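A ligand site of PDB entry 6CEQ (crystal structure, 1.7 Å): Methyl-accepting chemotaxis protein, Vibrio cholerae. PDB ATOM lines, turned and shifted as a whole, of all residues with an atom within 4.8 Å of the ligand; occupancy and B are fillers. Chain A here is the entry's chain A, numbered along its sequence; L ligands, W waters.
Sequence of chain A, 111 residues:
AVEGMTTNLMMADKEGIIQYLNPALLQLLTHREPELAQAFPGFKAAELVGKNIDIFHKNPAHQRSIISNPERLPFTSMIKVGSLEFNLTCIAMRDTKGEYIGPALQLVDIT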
ATOM      1  N   MET A  10      -2.700 -34.483  -4.515  1.00  0.00           N
ATOM      2  CA  MET A  10      -3.116 -33.873  -3.262  1.00  0.00           C
ATOM      3  C   MET A  10      -4.624 -34.008  -3.172  1.00  0.00           C
ATOM      4  O   MET A  10      -5.312 -33.766  -4.167  1.00  0.00           O
ATOM      5  CB  MET A  10      -2.677 -32.406  -3.240  1.00  0.00           C
ATOM      6  CG  MET A  10      -2.976 -31.638  -1.998  1.00  0.00           C
ATOM      7  SD  MET A  10      -1.975 -30.132  -2.045  1.00  0.00           S
ATOM      8  CE  MET A  10      -2.056 -29.641  -3.739  1.00  0.00           C
ATOM      9  N   MET A  11      -5.147 -34.404  -2.002  1.00  0.00           N
ATOM     10  CA  MET A  11      -6.594 -34.608  -1.820  1.00  0.00           C
ATOM     11  C   MET A  11      -7.143 -33.724  -0.710  1.00  0.00           C
ATOM     12  O   MET A  11      -6.479 -33.487   0.305  1.00  0.00           O
ATOM     13  CB  MET A  11      -6.894 -36.090  -1.489  1.00  0.00           C
ATOM     14  CG  MET A  11      -6.456 -37.075  -2.561  1.00  0.00           C
ATOM     15  SD  MET A  11      -6.049 -38.705  -1.888  1.00  0.00           S
ATOM     16  CE  MET A  11      -7.307 -38.907  -0.630  1.00  0.00           C
ATOM     17  N   ALA A  12      -8.384 -33.242  -0.889  1.00  0.00           N
ATOM     18  CA  ALA A  12      -9.053 -32.449   0.140  1.00  0.00           C
ATOM     19  C   ALA A  12     -10.493 -32.938   0.310  1.00  0.00           C
ATOM     20  O   ALA A  12     -11.046 -33.624  -0.552  1.00  0.00           O
ATOM     21  CB  ALA A  12      -9.053 -30.955  -0.217  1.00  0.00           C
ATOM     22  N   ILE A  18      -7.255 -30.114   3.572  1.00  0.00           N
ATOM     23  CA  ILE A  18      -6.328 -31.026   2.917  1.00  0.00           C
ATOM     24  C   ILE A  18      -6.263 -32.320   3.714  1.00  0.00           C
ATOM     25  O   ILE A  18      -6.125 -32.306   4.937  1.00  0.00           O
ATOM     26  CB  ILE A  18      -4.944 -30.384   2.781  1.00  0.00           C
ATOM     27  CG1 ILE A  18      -5.002 -29.156   1.866  1.00  0.00           C
ATOM     28  CG2 ILE A  18      -3.970 -31.388   2.239  1.00  0.00           C
ATOM     29  CD1 ILE A  18      -3.715 -28.356   1.838  1.00  0.00           C
ATOM     30  N   PHE A  40       4.868 -18.085  -0.133  1.00  0.00           N
ATOM     31  CA  PHE A  40       4.055 -18.392   1.041  1.00  0.00           C
ATOM     32  C   PHE A  40       4.985 -18.487   2.247  1.00  0.00           C
ATOM     33  O   PHE A  40       5.374 -19.574   2.672  1.00  0.00           O
ATOM     34  CB  PHE A  40       3.285 -19.696   0.856  1.00  0.00           C
ATOM     35  CG  PHE A  40       2.392 -19.721  -0.369  1.00  0.00           C
ATOM     36  CD1 PHE A  40       2.833 -20.271  -1.554  1.00  0.00           C
ATOM     37  CD2 PHE A  40       1.136 -19.156  -0.328  1.00  0.00           C
ATOM     38  CE1 PHE A  40       2.019 -20.293  -2.668  1.00  0.00           C
ATOM     39  CE2 PHE A  40       0.307 -19.171  -1.438  1.00  0.00           C
ATOM     40  CZ  PHE A  40       0.764 -19.743  -2.618  1.00  0.00           C
ATOM     41  N   PHE A  43       5.560 -21.512   4.775  1.00  0.00           N
ATOM     42  CA  PHE A  43       5.224 -22.790   4.161  1.00  0.00           C
ATOM     43  C   PHE A  43       6.094 -23.937   4.672  1.00  0.00           C
ATOM     44  O   PHE A  43       7.324 -23.816   4.734  1.00  0.00           O
ATOM     45  CB  PHE A  43       5.371 -22.664   2.643  1.00  0.00           C
ATOM     46  CG  PHE A  43       4.979 -23.891   1.882  1.00  0.00           C
ATOM     47  CD1 PHE A  43       3.656 -24.104   1.518  1.00  0.00           C
ATOM     48  CD2 PHE A  43       5.930 -24.844   1.529  1.00  0.00           C
ATOM     49  CE1 PHE A  43       3.292 -25.227   0.806  1.00  0.00           C
ATOM     50  CE2 PHE A  43       5.566 -25.973   0.830  1.00  0.00           C
ATOM     51  CZ  PHE A  43       4.248 -26.173   0.464  1.00  0.00           C
ATOM     52  N   LEU A  48       0.931 -29.457   5.685  1.00  0.00           N
ATOM     53  CA  LEU A  48      -0.212 -29.029   4.883  1.00  0.00           C
ATOM     54  C   LEU A  48      -1.494 -29.775   5.219  1.00  0.00           C
ATOM     55  O   LEU A  48      -2.587 -29.205   5.137  1.00  0.00           O
ATOM     56  CB  LEU A  48       0.116 -29.227   3.397  1.00  0.00           C
ATOM     57  CG  LEU A  48       1.172 -28.315   2.788  1.00  0.00           C
ATOM     58  CD1 LEU A  48       1.409 -28.710   1.333  1.00  0.00           C
ATOM     59  CD2 LEU A  48       0.753 -26.861   2.870  1.00  0.00           C
ATOM     60  N   ILE A  53      -7.550 -25.189   2.185  1.00  0.00           N
ATOM     61  CA  ILE A  53      -6.946 -24.728   0.953  1.00  0.00           C
ATOM     62  C   ILE A  53      -7.139 -23.235   0.723  1.00  0.00           C
ATOM     63  O   ILE A  53      -6.354 -22.617  -0.011  1.00  0.00           O
ATOM     64  CB  ILE A  53      -7.509 -25.518  -0.257  1.00  0.00           C
ATOM     65  CG1 ILE A  53      -9.006 -25.219  -0.437  1.00  0.00           C
ATOM     66  CG2 ILE A  53      -7.315 -27.008  -0.057  1.00  0.00           C
ATOM     67  CD1 ILE A  53      -9.632 -25.885  -1.689  1.00  0.00           C
ATOM     68  N   PHE A  56      -4.183 -20.688   0.682  1.00  0.00           N
ATOM     69  CA  PHE A  56      -3.207 -20.595  -0.392  1.00  0.00           C
ATOM     70  C   PHE A  56      -3.762 -19.980  -1.655  1.00  0.00           C
ATOM     71  O   PHE A  56      -3.029 -19.814  -2.630  1.00  0.00           O
ATOM     72  CB  PHE A  56      -2.660 -22.002  -0.695  1.00  0.00           C
ATOM     73  CG  PHE A  56      -2.112 -22.700   0.505  1.00  0.00           C
ATOM     74  CD1 PHE A  56      -0.859 -22.372   0.980  1.00  0.00           C
ATOM     75  CD2 PHE A  56      -2.860 -23.647   1.167  1.00  0.00           C
ATOM     76  CE1 PHE A  56      -0.343 -23.012   2.098  1.00  0.00           C
ATOM     77  CE2 PHE A  56      -2.350 -24.285   2.278  1.00  0.00           C
ATOM     78  CZ  PHE A  56      -1.097 -23.950   2.740  1.00  0.00           C
ATOM     79  N   HIS A  57      -5.041 -19.621  -1.658  1.00  0.00           N
ATOM     80  CA  HIS A  57      -5.711 -19.142  -2.860  1.00  0.00           C
ATOM     81  C   HIS A  57      -6.017 -17.658  -2.710  1.00  0.00           C
ATOM     82  O   HIS A  57      -6.642 -17.248  -1.733  1.00  0.00           O
ATOM     83  CB  HIS A  57      -6.984 -19.936  -3.097  1.00  0.00           C
ATOM     84  CG  HIS A  57      -6.741 -21.378  -3.376  1.00  0.00           C
ATOM     85  ND1 HIS A  57      -7.650 -22.373  -3.035  1.00  0.00           N
ATOM     86  CD2 HIS A  57      -5.722 -22.008  -4.005  1.00  0.00           C
ATOM     87  CE1 HIS A  57      -7.180 -23.531  -3.414  1.00  0.00           C
ATOM     88  NE2 HIS A  57      -6.013 -23.345  -4.020  1.00  0.00           N
ATOM     89  N   LYS A  58      -5.609 -16.871  -3.706  1.00  0.00           N
ATOM     90  CA  LYS A  58      -5.757 -15.425  -3.613  1.00  0.00           C
ATOM     91  C   LYS A  58      -7.220 -15.010  -3.628  1.00  0.00           C
ATOM     92  O   LYS A  58      -7.617 -14.088  -2.899  1.00  0.00           O
ATOM     93  CB  LYS A  58      -4.968 -14.732  -4.711  1.00  0.00           C
ATOM     94  CG  LYS A  58      -5.166 -15.278  -6.104  1.00  0.00           C
ATOM     95  CD  LYS A  58      -4.506 -14.380  -7.134  1.00  0.00           C
ATOM     96  CE  LYS A  58      -4.479 -15.023  -8.510  1.00  0.00           C
ATOM     97  NZ  LYS A  58      -3.913 -14.115  -9.543  1.00  0.00           N
ATOM     98  N   HIS A  62     -13.279 -18.578  -5.573  1.00  0.00           N
ATOM     99  CA  HIS A  62     -13.165 -19.137  -6.910  1.00  0.00           C
ATOM    100  C   HIS A  62     -12.926 -20.642  -6.850  1.00  0.00           C
ATOM    101  O   HIS A  62     -13.704 -21.437  -7.395  1.00  0.00           O
ATOM    102  CB  HIS A  62     -12.034 -18.425  -7.662  1.00  0.00           C
ATOM    103  CG  HIS A  62     -11.632 -19.086  -8.932  1.00  0.00           C
ATOM    104  ND1 HIS A  62     -12.516 -19.324  -9.969  1.00  0.00           N
ATOM    105  CD2 HIS A  62     -10.426 -19.530  -9.354  1.00  0.00           C
ATOM    106  CE1 HIS A  62     -11.869 -19.901 -10.963  1.00  0.00           C
ATOM    107  NE2 HIS A  62     -10.601 -20.032 -10.623  1.00  0.00           N
ATOM    108  N   GLN A  63     -11.870 -21.068  -6.149  1.00  0.00           N
ATOM    109  CA  GLN A  63     -11.603 -22.488  -6.002  1.00  0.00           C
ATOM    110  C   GLN A  63     -12.723 -23.186  -5.228  1.00  0.00           C
ATOM    111  O   GLN A  63     -13.028 -24.356  -5.499  1.00  0.00           O
ATOM    112  CB  GLN A  63     -10.257 -22.717  -5.317  1.00  0.00           C
ATOM    113  CG  GLN A  63      -9.066 -22.541  -6.218  1.00  0.00           C
ATOM    114  CD  GLN A  63      -8.561 -21.114  -6.279  1.00  0.00           C
ATOM    115  OE1 GLN A  63      -9.202 -20.184  -5.781  1.00  0.00           O
ATOM    116  NE2 GLN A  63      -7.366 -20.942  -6.844  1.00  0.00           N
ATOM    117  N   ILE A  66     -15.295 -24.185  -7.582  1.00  0.00           N
ATOM    118  CA  ILE A  66     -14.861 -25.315  -8.402  1.00  0.00           C
ATOM    119  C   ILE A  66     -15.041 -26.629  -7.637  1.00  0.00           C
ATOM    120  O   ILE A  66     -15.606 -27.593  -8.162  1.00  0.00           O
ATOM    121  CB  ILE A  66     -13.402 -25.129  -8.868  1.00  0.00           C
ATOM    122  CG1 ILE A  66     -13.274 -23.942  -9.827  1.00  0.00           C
ATOM    123  CG2 ILE A  66     -12.886 -26.408  -9.541  1.00  0.00           C
ATOM    124  CD1 ILE A  66     -11.846 -23.539 -10.102  1.00  0.00           C
ATOM    125  N   ILE A  67     -14.643 -26.669  -6.363  1.00  0.00           N
ATOM    126  CA  ILE A  67     -14.660 -27.944  -5.651  1.00  0.00           C
ATOM    127  C   ILE A  67     -16.006 -28.208  -4.988  1.00  0.00           C
ATOM    128  O   ILE A  67     -16.227 -29.311  -4.466  1.00  0.00           O
ATOM    129  CB  ILE A  67     -13.544 -28.040  -4.595  1.00  0.00           C
ATOM    130  CG1 ILE A  67     -13.841 -27.159  -3.377  1.00  0.00           C
ATOM    131  CG2 ILE A  67     -12.196 -27.694  -5.218  1.00  0.00           C
ATOM    132  CD1 ILE A  67     -13.096 -27.578  -2.114  1.00  0.00           C
ATOM    133  N   PHE A  75     -11.805 -30.411 -13.819  1.00  0.00           N
ATOM    134  CA  PHE A  75     -11.351 -29.054 -14.101  1.00  0.00           C
ATOM    135  C   PHE A  75      -9.866 -29.093 -14.417  1.00  0.00           C
ATOM    136  O   PHE A  75      -9.100 -29.768 -13.732  1.00  0.00           O
ATOM    137  CB  PHE A  75     -11.631 -28.128 -12.901  1.00  0.00           C
ATOM    138  CG  PHE A  75     -11.145 -26.724 -13.082  1.00  0.00           C
ATOM    139  CD1 PHE A  75     -11.986 -25.753 -13.593  1.00  0.00           C
ATOM    140  CD2 PHE A  75      -9.852 -26.375 -12.731  1.00  0.00           C
ATOM    141  CE1 PHE A  75     -11.545 -24.452 -13.761  1.00  0.00           C
ATOM    142  CE2 PHE A  75      -9.405 -25.067 -12.888  1.00  0.00           C
ATOM    143  CZ  PHE A  75     -10.250 -24.118 -13.401  1.00  0.00           C
ATOM    144  N   SER A  77      -6.341 -26.564 -15.661  1.00  0.00           N
ATOM    145  CA  SER A  77      -5.824 -25.205 -15.786  1.00  0.00           C
ATOM    146  C   SER A  77      -4.314 -25.244 -15.654  1.00  0.00           C
ATOM    147  O   SER A  77      -3.729 -26.213 -15.157  1.00  0.00           O
ATOM    148  CB  SER A  77      -6.431 -24.292 -14.708  1.00  0.00           C
ATOM    149  OG  SER A  77      -6.198 -22.931 -14.996  1.00  0.00           O
ATOM    150  N   MET A  78      -3.672 -24.169 -16.104  1.00  0.00           N
ATOM    151  CA  MET A  78      -2.268 -23.927 -15.844  1.00  0.00           C
ATOM    152  C   MET A  78      -2.186 -22.899 -14.721  1.00  0.00           C
ATOM    153  O   MET A  78      -2.900 -21.896 -14.746  1.00  0.00           O
ATOM    154  CB  MET A  78      -1.552 -23.434 -17.108  1.00  0.00           C
ATOM    155  CG  MET A  78      -0.120 -23.060 -16.879  1.00  0.00           C
ATOM    156  SD  MET A  78      -0.062 -21.284 -16.597  1.00  0.00           S
ATOM    157  CE  MET A  78       1.097 -21.214 -15.265  1.00  0.00           C
ATOM    158  N   ILE A  79      -1.358 -23.184 -13.708  1.00  0.00           N
ATOM    159  CA  ILE A  79      -1.294 -22.313 -12.544  1.00  0.00           C
ATOM    160  C   ILE A  79       0.156 -21.932 -12.256  1.00  0.00           C
ATOM    161  O   ILE A  79       1.098 -22.671 -12.545  1.00  0.00           O
ATOM    162  CB  ILE A  79      -1.933 -22.958 -11.290  1.00  0.00           C
ATOM    163  CG1 ILE A  79      -1.132 -24.174 -10.819  1.00  0.00           C
ATOM    164  CG2 ILE A  79      -3.389 -23.346 -11.588  1.00  0.00           C
ATOM    165  CD1 ILE A  79      -1.531 -24.625  -9.426  1.00  0.00           C
ATOM    166  N   LYS A  80       0.319 -20.721 -11.720  1.00  0.00           N
ATOM    167  CA  LYS A  80       1.594 -20.235 -11.217  1.00  0.00           C
ATOM    168  C   LYS A  80       1.548 -20.257  -9.697  1.00  0.00           C
ATOM    169  O   LYS A  80       0.633 -19.699  -9.095  1.00  0.00           O
ATOM    170  CB  LYS A  80       1.887 -18.807 -11.692  1.00  0.00           C
ATOM    171  CG  LYS A  80       2.069 -18.686 -13.188  1.00  0.00           C
ATOM    172  CD  LYS A  80       2.419 -17.280 -13.627  1.00  0.00           C
ATOM    173  CE  LYS A  80       2.590 -17.226 -15.148  1.00  0.00           C
ATOM    174  NZ  LYS A  80       2.826 -15.849 -15.655  1.00  0.00           N
ATOM    175  N   VAL A  81       2.524 -20.917  -9.093  1.00  0.00           N
ATOM    176  CA  VAL A  81       2.648 -21.016  -7.641  1.00  0.00           C
ATOM    177  C   VAL A  81       4.002 -20.394  -7.324  1.00  0.00           C
ATOM    178  O   VAL A  81       5.040 -21.065  -7.423  1.00  0.00           O
ATOM    179  CB  VAL A  81       2.543 -22.468  -7.148  1.00  0.00           C
ATOM    180  CG1 VAL A  81       2.500 -22.509  -5.636  1.00  0.00           C
ATOM    181  CG2 VAL A  81       1.323 -23.130  -7.736  1.00  0.00           C
ATOM    182  N   LEU A  88      -2.615 -28.260 -13.981  1.00  0.00           N
ATOM    183  CA  LEU A  88      -3.450 -28.739 -12.898  1.00  0.00           C
ATOM    184  C   LEU A  88      -4.629 -29.542 -13.413  1.00  0.00           C
ATOM    185  O   LEU A  88      -5.289 -29.129 -14.381  1.00  0.00           O
ATOM    186  CB  LEU A  88      -3.963 -27.564 -12.056  1.00  0.00           C
ATOM    187  CG  LEU A  88      -4.997 -27.832 -10.964  1.00  0.00           C
ATOM    188  CD1 LEU A  88      -4.774 -26.853  -9.811  1.00  0.00           C
ATOM    189  CD2 LEU A  88      -6.433 -27.703 -11.469  1.00  0.00           C
ATOM    190  N   CYS A  90      -8.143 -31.304 -11.619  1.00  0.00           N
ATOM    191  CA  CYS A  90      -8.960 -31.514 -10.437  1.00  0.00           C
ATOM    192  C   CYS A  90     -10.110 -32.447 -10.788  1.00  0.00           C
ATOM    193  O   CYS A  90     -10.870 -32.172 -11.712  1.00  0.00           O
ATOM    194  CB  CYS A  90      -9.496 -30.176  -9.917  1.00  0.00           C
ATOM    195  SG  CYS A  90     -10.382 -30.291  -8.352  1.00  0.00           S
ATOM    196  N   PRO A 103     -12.257 -32.993  -3.657  1.00  0.00           N
ATOM    197  CA  PRO A 103     -11.431 -32.954  -4.874  1.00  0.00           C
ATOM    198  C   PRO A 103     -10.110 -33.682  -4.696  1.00  0.00           C
ATOM    199  O   PRO A 103      -9.518 -33.705  -3.603  1.00  0.00           O
ATOM    200  CB  PRO A 103     -11.198 -31.457  -5.072  1.00  0.00           C
ATOM    201  CG  PRO A 103     -11.165 -30.913  -3.657  1.00  0.00           C
ATOM    202  CD  PRO A 103     -12.155 -31.738  -2.881  1.00  0.00           C
ATOM    203  N   LEU A 105      -6.367 -33.503  -6.712  1.00  0.00           N
ATOM    204  CA  LEU A 105      -5.587 -32.661  -7.589  1.00  0.00           C
ATOM    205  C   LEU A 105      -4.375 -33.420  -8.077  1.00  0.00           C
ATOM    206  O   LEU A 105      -3.652 -34.028  -7.266  1.00  0.00           O
ATOM    207  CB  LEU A 105      -5.089 -31.409  -6.871  1.00  0.00           C
ATOM    208  CG  LEU A 105      -5.770 -30.057  -6.727  1.00  0.00           C
ATOM    209  CD1 LEU A 105      -4.666 -29.056  -6.485  1.00  0.00           C
ATOM    210  CD2 LEU A 105      -6.585 -29.666  -7.956  1.00  0.00           C
HETATM  211  C1  LIG L   1      -4.864 -22.984  -8.175  1.00  0.00           C
HETATM  212  C2  LIG L   1      -7.628 -26.211  -5.849  1.00  0.00           C
HETATM  213  C3  LIG L   1      -3.844 -26.998  -2.852  1.00  0.00           C
HETATM  214  C4  LIG L   1      -2.202 -22.612  -4.121  1.00  0.00           C
HETATM  215  C5  LIG L   1      -5.846 -23.890  -7.878  1.00  0.00           C
HETATM  216  C6  LIG L   1      -6.884 -24.282  -8.760  1.00  0.00           C
HETATM  217  C7  LIG L   1      -7.664 -25.192  -8.113  1.00  0.00           C
HETATM  218  C8  LIG L   1      -7.129 -25.367  -6.818  1.00  0.00           C
HETATM  219  C9  LIG L   1      -8.882 -25.875  -8.680  1.00  0.00           C
HETATM  220  C10 LIG L   1      -7.082 -23.779 -10.166  1.00  0.00           C
HETATM  221  C11 LIG L   1      -7.692 -22.378 -10.124  1.00  0.00           C
HETATM  222  C12 LIG L   1      -7.735 -21.811 -11.523  1.00  0.00           C
HETATM  223  O1  LIG L   1      -6.863 -22.140 -12.360  1.00  0.00           O
HETATM  224  O2  LIG L   1      -8.636 -21.007 -11.846  1.00  0.00           O
HETATM  225  C13 LIG L   1      -6.773 -26.755  -4.874  1.00  0.00           C
HETATM  226  C14 LIG L   1      -7.099 -27.914  -4.128  1.00  0.00           C
HETATM  227  C15 LIG L   1      -6.060 -28.157  -3.276  1.00  0.00           C
HETATM  228  C16 LIG L   1      -5.065 -27.088  -3.534  1.00  0.00           C
HETATM  229  C17 LIG L   1      -8.362 -28.729  -4.248  1.00  0.00           C
HETATM  230  C18 LIG L   1      -5.943 -29.257  -2.307  1.00  0.00           C
HETATM  231  C19 LIG L   1      -6.300 -30.490  -2.648  1.00  0.00           C
HETATM  232  C20 LIG L   1      -3.055 -25.850  -2.899  1.00  0.00           C
HETATM  233  C21 LIG L   1      -1.893 -25.600  -2.148  1.00  0.00           C
HETATM  234  C22 LIG L   1      -1.421 -24.346  -2.511  1.00  0.00           C
HETATM  235  C23 LIG L   1      -2.314 -23.835  -3.501  1.00  0.00           C
HETATM  236  C24 LIG L   1      -1.279 -26.523  -1.135  1.00  0.00           C
HETATM  237  C25 LIG L   1      -0.228 -23.673  -1.980  1.00  0.00           C
HETATM  238  C26 LIG L   1       0.880 -24.370  -1.746  1.00  0.00           C
HETATM  239  C27 LIG L   1      -2.756 -22.409  -5.387  1.00  0.00           C
HETATM  240  C28 LIG L   1      -2.319 -21.333  -6.276  1.00  0.00           C
HETATM  241  C29 LIG L   1      -3.058 -21.428  -7.401  1.00  0.00           C
HETATM  242  C30 LIG L   1      -3.947 -22.584  -7.209  1.00  0.00           C
HETATM  243  C31 LIG L   1      -1.256 -20.307  -5.982  1.00  0.00           C
HETATM  244  C32 LIG L   1      -2.979 -20.540  -8.614  1.00  0.00           C
HETATM  245  C33 LIG L   1      -3.300 -19.102  -8.211  1.00  0.00           C
HETATM  246  C34 LIG L   1      -4.663 -19.043  -7.573  1.00  0.00           C
HETATM  247  O3  LIG L   1      -4.775 -18.735  -6.365  1.00  0.00           O
HETATM  248  O4  LIG L   1      -5.678 -19.308  -8.246  1.00  0.00           O
HETATM  249  N1  LIG L   1      -6.027 -24.575  -6.700  1.00  0.00           N
HETATM  250  N2  LIG L   1      -5.566 -26.294  -4.500  1.00  0.00           N
HETATM  251  N3  LIG L   1      -3.285 -24.774  -3.714  1.00  0.00           N
HETATM  252  N4  LIG L   1      -3.728 -23.113  -5.997  1.00  0.00           N
HETATM  253 FE1  LIG L   1      -4.624 -24.603  -5.298  1.00  0.00          FE
HETATM  254  O   HOH W   1      -7.798 -17.888  -6.110  1.00  0.00           O
HETATM  255  O   HOH W   2      -0.478 -17.565  -8.871  1.00  0.00           O
HETATM  256  O   HOH W   3      -3.117 -26.264  -6.520  1.00  0.00           O
HETATM  257  O   HOH W   4      -5.142 -20.618 -14.098  1.00  0.00           O
HETATM  258  O   HOH W   5      -2.539 -17.698  -4.077  1.00  0.00           O
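An oxygen (O3) of the ligand is in hydrogen-bond range of the backbone NH (N) of Lys 58 (3.4 Å).
The side-chain hydroxyl (OG) of Ser 77 is in hydrogen-bond range of an oxygen (O1) of the ligand (2.8 Å).
A ring nitrogen (NE2) of His 57 is bound to an iron atom (FE1) of the ligand, 2.3 Å away.
An oxygen (O4) of the ligand is in hydrogen-bond range of the side-chain amide nitrogen (NE2) of Gln 63, 2.7 Å away.
An oxygen (O2) of the ligand is in hydrogen-bond range of a ring nitrogen (NE2) of His 62 (2.5 Å).
Residues that only touch the ligand: Phe 56 (3.2 Å), Met 10 (3.3 Å), Ile 53 (3.5 Å), Leu 88 (3.5 Å), Leu 105 (3.5 Å), Pro 103 (3.6 Å), Phe 43 (3.6 Å), Lys 80 (3.7 Å), Ala 12 (3.7 Å), Ile 79 (3.7 Å), Phe 75 (3.8 Å), Met 11 (3.9 Å) and Phe 40 (3.96 Å).
Hydrophobic or aromatic side chains within 4 Å of the ligand: Met 10, Ala 12, Phe 40, Phe 43, Ile 53, Phe 56, His 57, His 62, Phe 75, Ile 79, Leu 88, Pro 103 and Leu 105.
Within 4 Å of the ligand: Met 10, Met 11, Ala 12, Phe 40, Phe 43, Ile 53, Phe 56, His 57, Lys 58, His 62, Gln 63, Phe 75, Ser 77, Ile 79, Lys 80, Leu 88, Pro 103 and Leu 105.
Water W4 lies within hydrogen-bond range of the backbone carbonyl oxygen (O) of Met 78 (2.7 Å), the side-chain hydroxyl (OG) of Ser 77 (2.7 Å) and an oxygen (O1) of the ligand (2.9 Å).
Water W1 lies within hydrogen-bond range of the side-chain amide oxygen (OE1) of Gln 63 (2.7 Å), an oxygen (O3) of the ligand (3.1 Å) and the backbone NH (N) of Lys 58 (3.4 Å).
Water W5 lies within hydrogen-bond range of O of Phe 56 (2.6 Å), N of Lys 58 (3.2 Å) and O3 of the ligand (3.4 Å).
ND1 of His 57 lies within hydrogen-bond range of O of Ile 53, 3.3 Å away.
The backbone carbonyl oxygen of Pro 103 is in hydrogen-bond range of the backbone NH of Ala 12 (3.0 Å).
The backbone NH (N) of Cys 90 is in hydrogen-bond range of the backbone carbonyl oxygen (O) of Phe 75.
The backbone carbonyl oxygen (O) of Ser 77 is in hydrogen-bond range of the backbone NH (N) of Leu 88 (2.6 Å).
O of Met 10 lies within hydrogen-bond range of N of Leu 105, 2.8 Å away.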
